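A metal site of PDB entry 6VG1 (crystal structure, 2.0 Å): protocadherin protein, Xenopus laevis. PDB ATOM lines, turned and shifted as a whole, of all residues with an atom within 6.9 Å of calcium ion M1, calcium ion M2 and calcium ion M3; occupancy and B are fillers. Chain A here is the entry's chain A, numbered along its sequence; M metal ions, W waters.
The backbone NH of Arg 172 lies close to the side-chain carboxylate of Glu 114.
The backbone carbonyl oxygen (O) of Leu 203 sits at hydrogen-bond distance from the backbone NH (N) of Glu 114, 3.0 Å away.
OE2 of Glu 173 lies close to NH2 of Arg 172 (3.5 Å).
The side-chain carboxylate of Asp 204 sits at hydrogen-bond distance from the side-chain amide nitrogen of Asn 244, 3.1 Å away.
NE of Arg 172 lies close to OD1 of Asp 204.
OD2 of Asp 204 is in hydrogen-bond range of N of Glu 241 (3.4 Å).
OD1 of Asp 294 is in hydrogen-bond range of N of Leu 300 (2.7 Å).
OG of Ser 174 is in hydrogen-bond range of OD2 of Asp 171 (3.1 Å).
Within 4 Å of calcium ion M1: Glu 114, Asp 171, Glu 173, Asp 207 and Asn 208.
Within 4 Å of calcium ion M2: Glu 114, Glu 173, Asp 204, Phe 205, Asp 207 and Asp 240.
Along chain A the residues within 4 Å of calcium ion M2 span positions 114 to 240.
The nearest printed residue that does not touch calcium ion M2 is Asn 208 (4.2 Å).
Within 4 Å of calcium ion M3: Asn 206, Asn 208, Asp 238, Asp 240, Asn 244 and Asp 294.
The nearest printed residue that does not touch calcium ion M3 is Leu 300 (4.4 Å).
Calcium ion M1 is bound by the side-chain carboxylate (OD2) of Asp 207 (2.2 Å), water W2 (2.3 Å), the side-chain carboxylate (OE1) of Glu 114 (2.3 Å), the side-chain carboxylate (OE1) of Glu 173 (2.3 Å), the side-chain carboxylate (OD1) of Asp 171 (2.5 Å) and water W1 (2.6 Å).
Calcium ion M1 has six donor atoms within binding distance.
Slightly farther from calcium ion M1 lies the side-chain carboxylate (OD1) of Asp 207 (3.1 Å).
Calcium ion M2 is bound by OE2 of Glu 173 (2.3 Å), OE2 of Glu 114 (2.4 Å), OD1 of Asp 204 (2.4 Å), OD1 of Asp 207 (2.4 Å), OD2 of Asp 240 (2.4 Å) and O of Phe 205 (2.4 Å).
Slightly farther from calcium ion M2 lies the side-chain carboxylate (OE1) of Glu 173 (3.0 Å).
O of Asn 208 is bound to calcium ion M3, 2.3 Å away.
OD2 of Asp 294 is bound to calcium ion M3, at 2.4 Å.
Calcium ion M3 is bound by OD1 of Asp 240 (2.4 Å).
OD1 of Asp 238 is bound to calcium ion M3 (2.4 Å).
O of Asn 244 is bound to calcium ion M3.
The side-chain amide oxygen (OD1) of Asn 206 is bound to calcium ion M3.
Calcium ion M3 is bound by the side-chain carboxylate (OD2) of Asp 238, at 2.4 Å.
Calcium ion M3 has seven donor atoms within binding distance.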
ATOM      1  N   GLU A 114      18.099   3.269  -8.892  1.00  0.00           N
ATOM      2  CA  GLU A 114      17.400   4.495  -9.277  1.00  0.00           C
ATOM      3  C   GLU A 114      15.984   4.526  -8.716  1.00  0.00           C
ATOM      4  O   GLU A 114      15.364   5.599  -8.682  1.00  0.00           O
ATOM      5  CB  GLU A 114      17.367   4.642 -10.795  1.00  0.00           C
ATOM      6  CG  GLU A 114      16.302   3.839 -11.502  1.00  0.00           C
ATOM      7  CD  GLU A 114      16.366   4.054 -13.009  1.00  0.00           C
ATOM      8  OE1 GLU A 114      16.223   5.216 -13.456  1.00  0.00           O
ATOM      9  OE2 GLU A 114      16.576   3.056 -13.743  1.00  0.00           O
ATOM     10  N   LEU A 170      16.394   9.540  -8.126  1.00  0.00           N
ATOM     11  CA  LEU A 170      17.424   9.304  -9.127  1.00  0.00           C
ATOM     12  C   LEU A 170      16.813   8.870 -10.462  1.00  0.00           C
ATOM     13  O   LEU A 170      15.685   8.385 -10.520  1.00  0.00           O
ATOM     14  CB  LEU A 170      18.424   8.242  -8.670  1.00  0.00           C
ATOM     15  CG  LEU A 170      19.311   8.591  -7.484  1.00  0.00           C
ATOM     16  CD1 LEU A 170      20.180   7.389  -7.161  1.00  0.00           C
ATOM     17  CD2 LEU A 170      20.152   9.817  -7.723  1.00  0.00           C
ATOM     18  N   ASP A 171      17.595   9.041 -11.536  1.00  0.00           N
ATOM     19  CA  ASP A 171      17.228   8.572 -12.874  1.00  0.00           C
ATOM     20  C   ASP A 171      18.522   8.141 -13.547  1.00  0.00           C
ATOM     21  O   ASP A 171      19.298   8.982 -14.008  1.00  0.00           O
ATOM     22  CB  ASP A 171      16.512   9.665 -13.668  1.00  0.00           C
ATOM     23  CG  ASP A 171      16.074   9.180 -15.045  1.00  0.00           C
ATOM     24  OD1 ASP A 171      16.178   7.961 -15.320  1.00  0.00           O
ATOM     25  OD2 ASP A 171      15.603  10.030 -15.843  1.00  0.00           O
ATOM     26  N   ARG A 172      18.724   6.819 -13.651  1.00  0.00           N
ATOM     27  CA  ARG A 172      19.977   6.325 -14.229  1.00  0.00           C
ATOM     28  C   ARG A 172      20.138   6.730 -15.683  1.00  0.00           C
ATOM     29  O   ARG A 172      21.268   6.819 -16.175  1.00  0.00           O
ATOM     30  CB  ARG A 172      20.053   4.798 -14.092  1.00  0.00           C
ATOM     31  CG  ARG A 172      21.448   4.240 -14.338  1.00  0.00           C
ATOM     32  CD  ARG A 172      21.419   2.793 -14.814  1.00  0.00           C
ATOM     33  NE  ARG A 172      20.762   2.667 -16.120  1.00  0.00           N
ATOM     34  CZ  ARG A 172      21.404   2.733 -17.284  1.00  0.00           C
ATOM     35  NH1 ARG A 172      22.712   2.914 -17.327  1.00  0.00           N
ATOM     36  NH2 ARG A 172      20.721   2.603 -18.410  1.00  0.00           N
ATOM     37  N   GLU A 173      19.038   6.963 -16.398  1.00  0.00           N
ATOM     38  CA  GLU A 173      19.135   7.355 -17.797  1.00  0.00           C
ATOM     39  C   GLU A 173      19.641   8.788 -17.943  1.00  0.00           C
ATOM     40  O   GLU A 173      20.276   9.119 -18.942  1.00  0.00           O
ATOM     41  CB  GLU A 173      17.782   7.178 -18.478  1.00  0.00           C
ATOM     42  CG  GLU A 173      17.389   5.710 -18.727  1.00  0.00           C
ATOM     43  CD  GLU A 173      17.233   4.895 -17.451  1.00  0.00           C
ATOM     44  OE1 GLU A 173      16.852   5.471 -16.417  1.00  0.00           O
ATOM     45  OE2 GLU A 173      17.501   3.670 -17.493  1.00  0.00           O
ATOM     46  N   SER A 174      19.355   9.657 -16.956  1.00  0.00           N
ATOM     47  CA  SER A 174      19.918  10.997 -16.939  1.00  0.00           C
ATOM     48  C   SER A 174      21.349  10.992 -16.414  1.00  0.00           C
ATOM     49  O   SER A 174      22.244  11.598 -17.010  1.00  0.00           O
ATOM     50  CB  SER A 174      19.052  11.931 -16.080  1.00  0.00           C
ATOM     51  OG  SER A 174      17.770  12.139 -16.643  1.00  0.00           O
ATOM     52  N   LEU A 203      22.160   1.850  -9.937  1.00  0.00           N
ATOM     53  CA  LEU A 203      21.744   0.583 -10.501  1.00  0.00           C
ATOM     54  C   LEU A 203      20.413   0.729 -11.219  1.00  0.00           C
ATOM     55  O   LEU A 203      19.526   1.455 -10.761  1.00  0.00           O
ATOM     56  CB  LEU A 203      21.615  -0.478  -9.403  1.00  0.00           C
ATOM     57  CG  LEU A 203      22.887  -0.734  -8.591  1.00  0.00           C
ATOM     58  CD1 LEU A 203      22.603  -1.785  -7.526  1.00  0.00           C
ATOM     59  CD2 LEU A 203      24.033  -1.167  -9.473  1.00  0.00           C
ATOM     60  N   ASP A 204      20.275   0.036 -12.356  1.00  0.00           N
ATOM     61  CA  ASP A 204      19.149   0.299 -13.238  1.00  0.00           C
ATOM     62  C   ASP A 204      17.883  -0.403 -12.760  1.00  0.00           C
ATOM     63  O   ASP A 204      17.929  -1.535 -12.257  1.00  0.00           O
ATOM     64  CB  ASP A 204      19.446  -0.127 -14.670  1.00  0.00           C
ATOM     65  CG  ASP A 204      18.323   0.249 -15.638  1.00  0.00           C
ATOM     66  OD1 ASP A 204      18.138   1.454 -15.891  1.00  0.00           O
ATOM     67  OD2 ASP A 204      17.643  -0.669 -16.153  1.00  0.00           O
ATOM     68  N   PHE A 205      16.762   0.282 -12.910  1.00  0.00           N
ATOM     69  CA  PHE A 205      15.423  -0.270 -12.788  1.00  0.00           C
ATOM     70  C   PHE A 205      14.781  -0.218 -14.166  1.00  0.00           C
ATOM     71  O   PHE A 205      15.143   0.624 -14.999  1.00  0.00           O
ATOM     72  CB  PHE A 205      14.613   0.527 -11.763  1.00  0.00           C
ATOM     73  CG  PHE A 205      13.249  -0.036 -11.492  1.00  0.00           C
ATOM     74  CD1 PHE A 205      13.092  -1.313 -10.963  1.00  0.00           C
ATOM     75  CD2 PHE A 205      12.124   0.719 -11.736  1.00  0.00           C
ATOM     76  CE1 PHE A 205      11.836  -1.822 -10.712  1.00  0.00           C
ATOM     77  CE2 PHE A 205      10.865   0.219 -11.483  1.00  0.00           C
ATOM     78  CZ  PHE A 205      10.721  -1.052 -10.972  1.00  0.00           C
ATOM     79  N   ASN A 206      13.853  -1.139 -14.426  1.00  0.00           N
ATOM     80  CA  ASN A 206      13.177  -1.198 -15.726  1.00  0.00           C
ATOM     81  C   ASN A 206      11.948  -0.290 -15.689  1.00  0.00           C
ATOM     82  O   ASN A 206      10.810  -0.738 -15.619  1.00  0.00           O
ATOM     83  CB  ASN A 206      12.802  -2.630 -16.079  1.00  0.00           C
ATOM     84  CG  ASN A 206      12.245  -2.749 -17.487  1.00  0.00           C
ATOM     85  OD1 ASN A 206      12.784  -2.180 -18.437  1.00  0.00           O
ATOM     86  ND2 ASN A 206      11.148  -3.480 -17.619  1.00  0.00           N
ATOM     87  N   ASP A 207      12.223   1.014 -15.720  1.00  0.00           N
ATOM     88  CA  ASP A 207      11.188   2.029 -15.674  1.00  0.00           C
ATOM     89  C   ASP A 207      10.955   2.687 -17.021  1.00  0.00           C
ATOM     90  O   ASP A 207      10.276   3.721 -17.090  1.00  0.00           O
ATOM     91  CB  ASP A 207      11.554   3.090 -14.636  1.00  0.00           C
ATOM     92  CG  ASP A 207      12.971   3.608 -14.819  1.00  0.00           C
ATOM     93  OD1 ASP A 207      13.784   2.934 -15.492  1.00  0.00           O
ATOM     94  OD2 ASP A 207      13.274   4.697 -14.257  1.00  0.00           O
ATOM     95  N   ASN A 208      11.468   2.101 -18.099  1.00  0.00           N
ATOM     96  CA  ASN A 208      11.229   2.610 -19.439  1.00  0.00           C
ATOM     97  C   ASN A 208      10.779   1.480 -20.331  1.00  0.00           C
ATOM     98  O   ASN A 208      11.532   0.540 -20.594  1.00  0.00           O
ATOM     99  CB  ASN A 208      12.493   3.277 -19.996  1.00  0.00           C
ATOM    100  CG  ASN A 208      12.728   4.636 -19.405  1.00  0.00           C
ATOM    101  OD1 ASN A 208      13.668   4.843 -18.645  1.00  0.00           O
ATOM    102  ND2 ASN A 208      11.857   5.578 -19.749  1.00  0.00           N
ATOM    103  N   SER A 209       9.554   1.585 -20.846  1.00  0.00           N
ATOM    104  CA  SER A 209       9.077   0.655 -21.836  1.00  0.00           C
ATOM    105  C   SER A 209       9.729   0.980 -23.174  1.00  0.00           C
ATOM    106  O   SER A 209      10.133   2.122 -23.410  1.00  0.00           O
ATOM    107  CB  SER A 209       7.568   0.767 -21.967  1.00  0.00           C
ATOM    108  OG  SER A 209       7.201   2.143 -21.943  1.00  0.00           O
ATOM    109  N   PRO A 210       9.858  -0.005 -24.059  1.00  0.00           N
ATOM    110  CA  PRO A 210      10.400   0.289 -25.395  1.00  0.00           C
ATOM    111  C   PRO A 210       9.485   1.247 -26.151  1.00  0.00           C
ATOM    112  O   PRO A 210       8.332   1.476 -25.769  1.00  0.00           O
ATOM    113  CB  PRO A 210      10.461  -1.080 -26.087  1.00  0.00           C
ATOM    114  CG  PRO A 210       9.645  -2.002 -25.234  1.00  0.00           C
ATOM    115  CD  PRO A 210       9.622  -1.441 -23.843  1.00  0.00           C
ATOM    116  N   ASP A 238      15.103   1.085 -26.380  1.00  0.00           N
ATOM    117  CA  ASP A 238      14.818   1.054 -24.945  1.00  0.00           C
ATOM    118  C   ASP A 238      16.011   1.683 -24.227  1.00  0.00           C
ATOM    119  O   ASP A 238      17.140   1.196 -24.385  1.00  0.00           O
ATOM    120  CB  ASP A 238      14.600  -0.373 -24.443  1.00  0.00           C
ATOM    121  CG  ASP A 238      13.902  -0.422 -23.082  1.00  0.00           C
ATOM    122  OD1 ASP A 238      12.726  -0.838 -23.026  1.00  0.00           O
ATOM    123  OD2 ASP A 238      14.544  -0.062 -22.073  1.00  0.00           O
ATOM    124  N   PRO A 239      15.818   2.745 -23.458  1.00  0.00           N
ATOM    125  CA  PRO A 239      16.982   3.405 -22.824  1.00  0.00           C
ATOM    126  C   PRO A 239      17.576   2.618 -21.667  1.00  0.00           C
ATOM    127  O   PRO A 239      18.720   2.890 -21.297  1.00  0.00           O
ATOM    128  CB  PRO A 239      16.412   4.753 -22.363  1.00  0.00           C
ATOM    129  CG  PRO A 239      14.958   4.469 -22.109  1.00  0.00           C
ATOM    130  CD  PRO A 239      14.550   3.448 -23.150  1.00  0.00           C
ATOM    131  N   ASP A 240      16.835   1.662 -21.103  1.00  0.00           N
ATOM    132  CA  ASP A 240      17.302   0.931 -19.923  1.00  0.00           C
ATOM    133  C   ASP A 240      18.568   0.146 -20.265  1.00  0.00           C
ATOM    134  O   ASP A 240      18.990   0.053 -21.409  1.00  0.00           O
ATOM    135  CB  ASP A 240      16.210  -0.016 -19.415  1.00  0.00           C
ATOM    136  CG  ASP A 240      14.973   0.713 -18.848  1.00  0.00           C
ATOM    137  OD1 ASP A 240      13.839   0.365 -19.259  1.00  0.00           O
ATOM    138  OD2 ASP A 240      15.127   1.627 -17.994  1.00  0.00           O
ATOM    139  N   GLU A 241      19.155  -0.454 -19.224  1.00  0.00           N
ATOM    140  CA  GLU A 241      20.472  -1.081 -19.311  1.00  0.00           C
ATOM    141  C   GLU A 241      20.339  -2.584 -19.498  1.00  0.00           C
ATOM    142  O   GLU A 241      19.404  -3.213 -19.008  1.00  0.00           O
ATOM    143  CB  GLU A 241      21.304  -0.795 -18.055  1.00  0.00           C
ATOM    144  CG  GLU A 241      22.680  -1.433 -18.069  1.00  0.00           C
ATOM    145  CD  GLU A 241      23.439  -1.204 -16.765  1.00  0.00           C
ATOM    146  OE1 GLU A 241      23.009  -0.339 -15.955  1.00  0.00           O
ATOM    147  OE2 GLU A 241      24.462  -1.884 -16.532  1.00  0.00           O
ATOM    148  N   ALA A 243      19.654  -6.248 -20.058  1.00  0.00           N
ATOM    149  CA  ALA A 243      18.461  -6.991 -20.462  1.00  0.00           C
ATOM    150  C   ALA A 243      17.220  -6.094 -20.450  1.00  0.00           C
ATOM    151  O   ALA A 243      16.329  -6.249 -21.284  1.00  0.00           O
ATOM    152  CB  ALA A 243      18.255  -8.194 -19.539  1.00  0.00           C
ATOM    153  N   ASN A 244      17.142  -5.163 -19.500  1.00  0.00           N
ATOM    154  CA  ASN A 244      15.981  -4.290 -19.442  1.00  0.00           C
ATOM    155  C   ASN A 244      15.810  -3.436 -20.692  1.00  0.00           C
ATOM    156  O   ASN A 244      14.751  -2.853 -20.897  1.00  0.00           O
ATOM    157  CB  ASN A 244      16.057  -3.360 -18.230  1.00  0.00           C
ATOM    158  CG  ASN A 244      15.968  -4.126 -16.931  1.00  0.00           C
ATOM    159  OD1 ASN A 244      15.565  -5.288 -16.916  1.00  0.00           O
ATOM    160  ND2 ASN A 244      16.334  -3.489 -15.836  1.00  0.00           N
ATOM    161  N   GLY A 245      16.836  -3.363 -21.541  1.00  0.00           N
ATOM    162  CA  GLY A 245      16.779  -2.555 -22.731  1.00  0.00           C
ATOM    163  C   GLY A 245      16.914  -3.377 -24.004  1.00  0.00           C
ATOM    164  O   GLY A 245      17.026  -2.821 -25.103  1.00  0.00           O
ATOM    165  N   GLU A 246      16.932  -4.703 -23.848  1.00  0.00           N
ATOM    166  CA  GLU A 246      17.073  -5.621 -24.969  1.00  0.00           C
ATOM    167  C   GLU A 246      15.681  -6.016 -25.445  1.00  0.00           C
ATOM    168  O   GLU A 246      14.874  -6.512 -24.646  1.00  0.00           O
ATOM    169  CB  GLU A 246      17.891  -6.847 -24.547  1.00  0.00           C
ATOM    170  CG  GLU A 246      18.471  -7.657 -25.698  1.00  0.00           C
ATOM    171  CD  GLU A 246      19.484  -8.696 -25.234  1.00  0.00           C
ATOM    172  OE1 GLU A 246      19.774  -8.750 -24.017  1.00  0.00           O
ATOM    173  OE2 GLU A 246      19.993  -9.450 -26.092  1.00  0.00           O
ATOM    174  N   ASP A 294      10.742  -5.668 -23.812  1.00  0.00           N
ATOM    175  CA  ASP A 294      12.082  -5.806 -23.256  1.00  0.00           C
ATOM    176  C   ASP A 294      12.170  -7.092 -22.436  1.00  0.00           C
ATOM    177  O   ASP A 294      11.166  -7.596 -21.931  1.00  0.00           O
ATOM    178  CB  ASP A 294      12.479  -4.605 -22.396  1.00  0.00           C
ATOM    179  CG  ASP A 294      11.541  -4.359 -21.228  1.00  0.00           C
ATOM    180  OD1 ASP A 294      10.707  -5.233 -20.920  1.00  0.00           O
ATOM    181  OD2 ASP A 294      11.642  -3.269 -20.627  1.00  0.00           O
ATOM    182  N   MET A 295      13.390  -7.612 -22.300  1.00  0.00           N
ATOM    183  CA  MET A 295      13.612  -8.861 -21.579  1.00  0.00           C
ATOM    184  C   MET A 295      14.024  -8.534 -20.150  1.00  0.00           C
ATOM    185  O   MET A 295      15.193  -8.581 -19.763  1.00  0.00           O
ATOM    186  CB  MET A 295      14.653  -9.705 -22.301  1.00  0.00           C
ATOM    187  CG  MET A 295      14.151 -10.256 -23.610  1.00  0.00           C
ATOM    188  SD  MET A 295      15.366 -11.291 -24.438  1.00  0.00           S
ATOM    189  CE  MET A 295      16.538 -10.027 -24.961  1.00  0.00           C
ATOM    190  N   ALA A 296      13.017  -8.179 -19.353  1.00  0.00           N
ATOM    191  CA  ALA A 296      13.218  -7.827 -17.956  1.00  0.00           C
ATOM    192  C   ALA A 296      12.287  -8.658 -17.082  1.00  0.00           C
ATOM    193  O   ALA A 296      11.361  -9.327 -17.561  1.00  0.00           O
ATOM    194  CB  ALA A 296      12.975  -6.332 -17.709  1.00  0.00           C
ATOM    195  N   LEU A 300       8.152  -4.750 -20.208  1.00  0.00           N
ATOM    196  CA  LEU A 300       7.414  -3.606 -20.729  1.00  0.00           C
ATOM    197  C   LEU A 300       7.265  -3.755 -22.237  1.00  0.00           C
ATOM    198  O   LEU A 300       8.110  -4.347 -22.911  1.00  0.00           O
ATOM    199  CB  LEU A 300       8.137  -2.314 -20.383  1.00  0.00           C
ATOM    200  CG  LEU A 300       8.315  -2.115 -18.871  1.00  0.00           C
ATOM    201  CD1 LEU A 300       9.197  -0.956 -18.510  1.00  0.00           C
ATOM    202  CD2 LEU A 300       6.908  -1.972 -18.248  1.00  0.00           C
HETATM  203 CA    CA M   1      14.914   5.852 -15.191  1.00  0.00          CA
HETATM  204 CA    CA M   2      16.085   2.610 -16.007  1.00  0.00          CA
HETATM  205 CA    CA M   3      12.948  -1.300 -20.697  1.00  0.00          CA
HETATM  206  O   HOH W   1      13.637   7.215 -16.999  1.00  0.00           O
HETATM  207  O   HOH W   2      14.231   7.428 -13.722  1.00  0.00           O
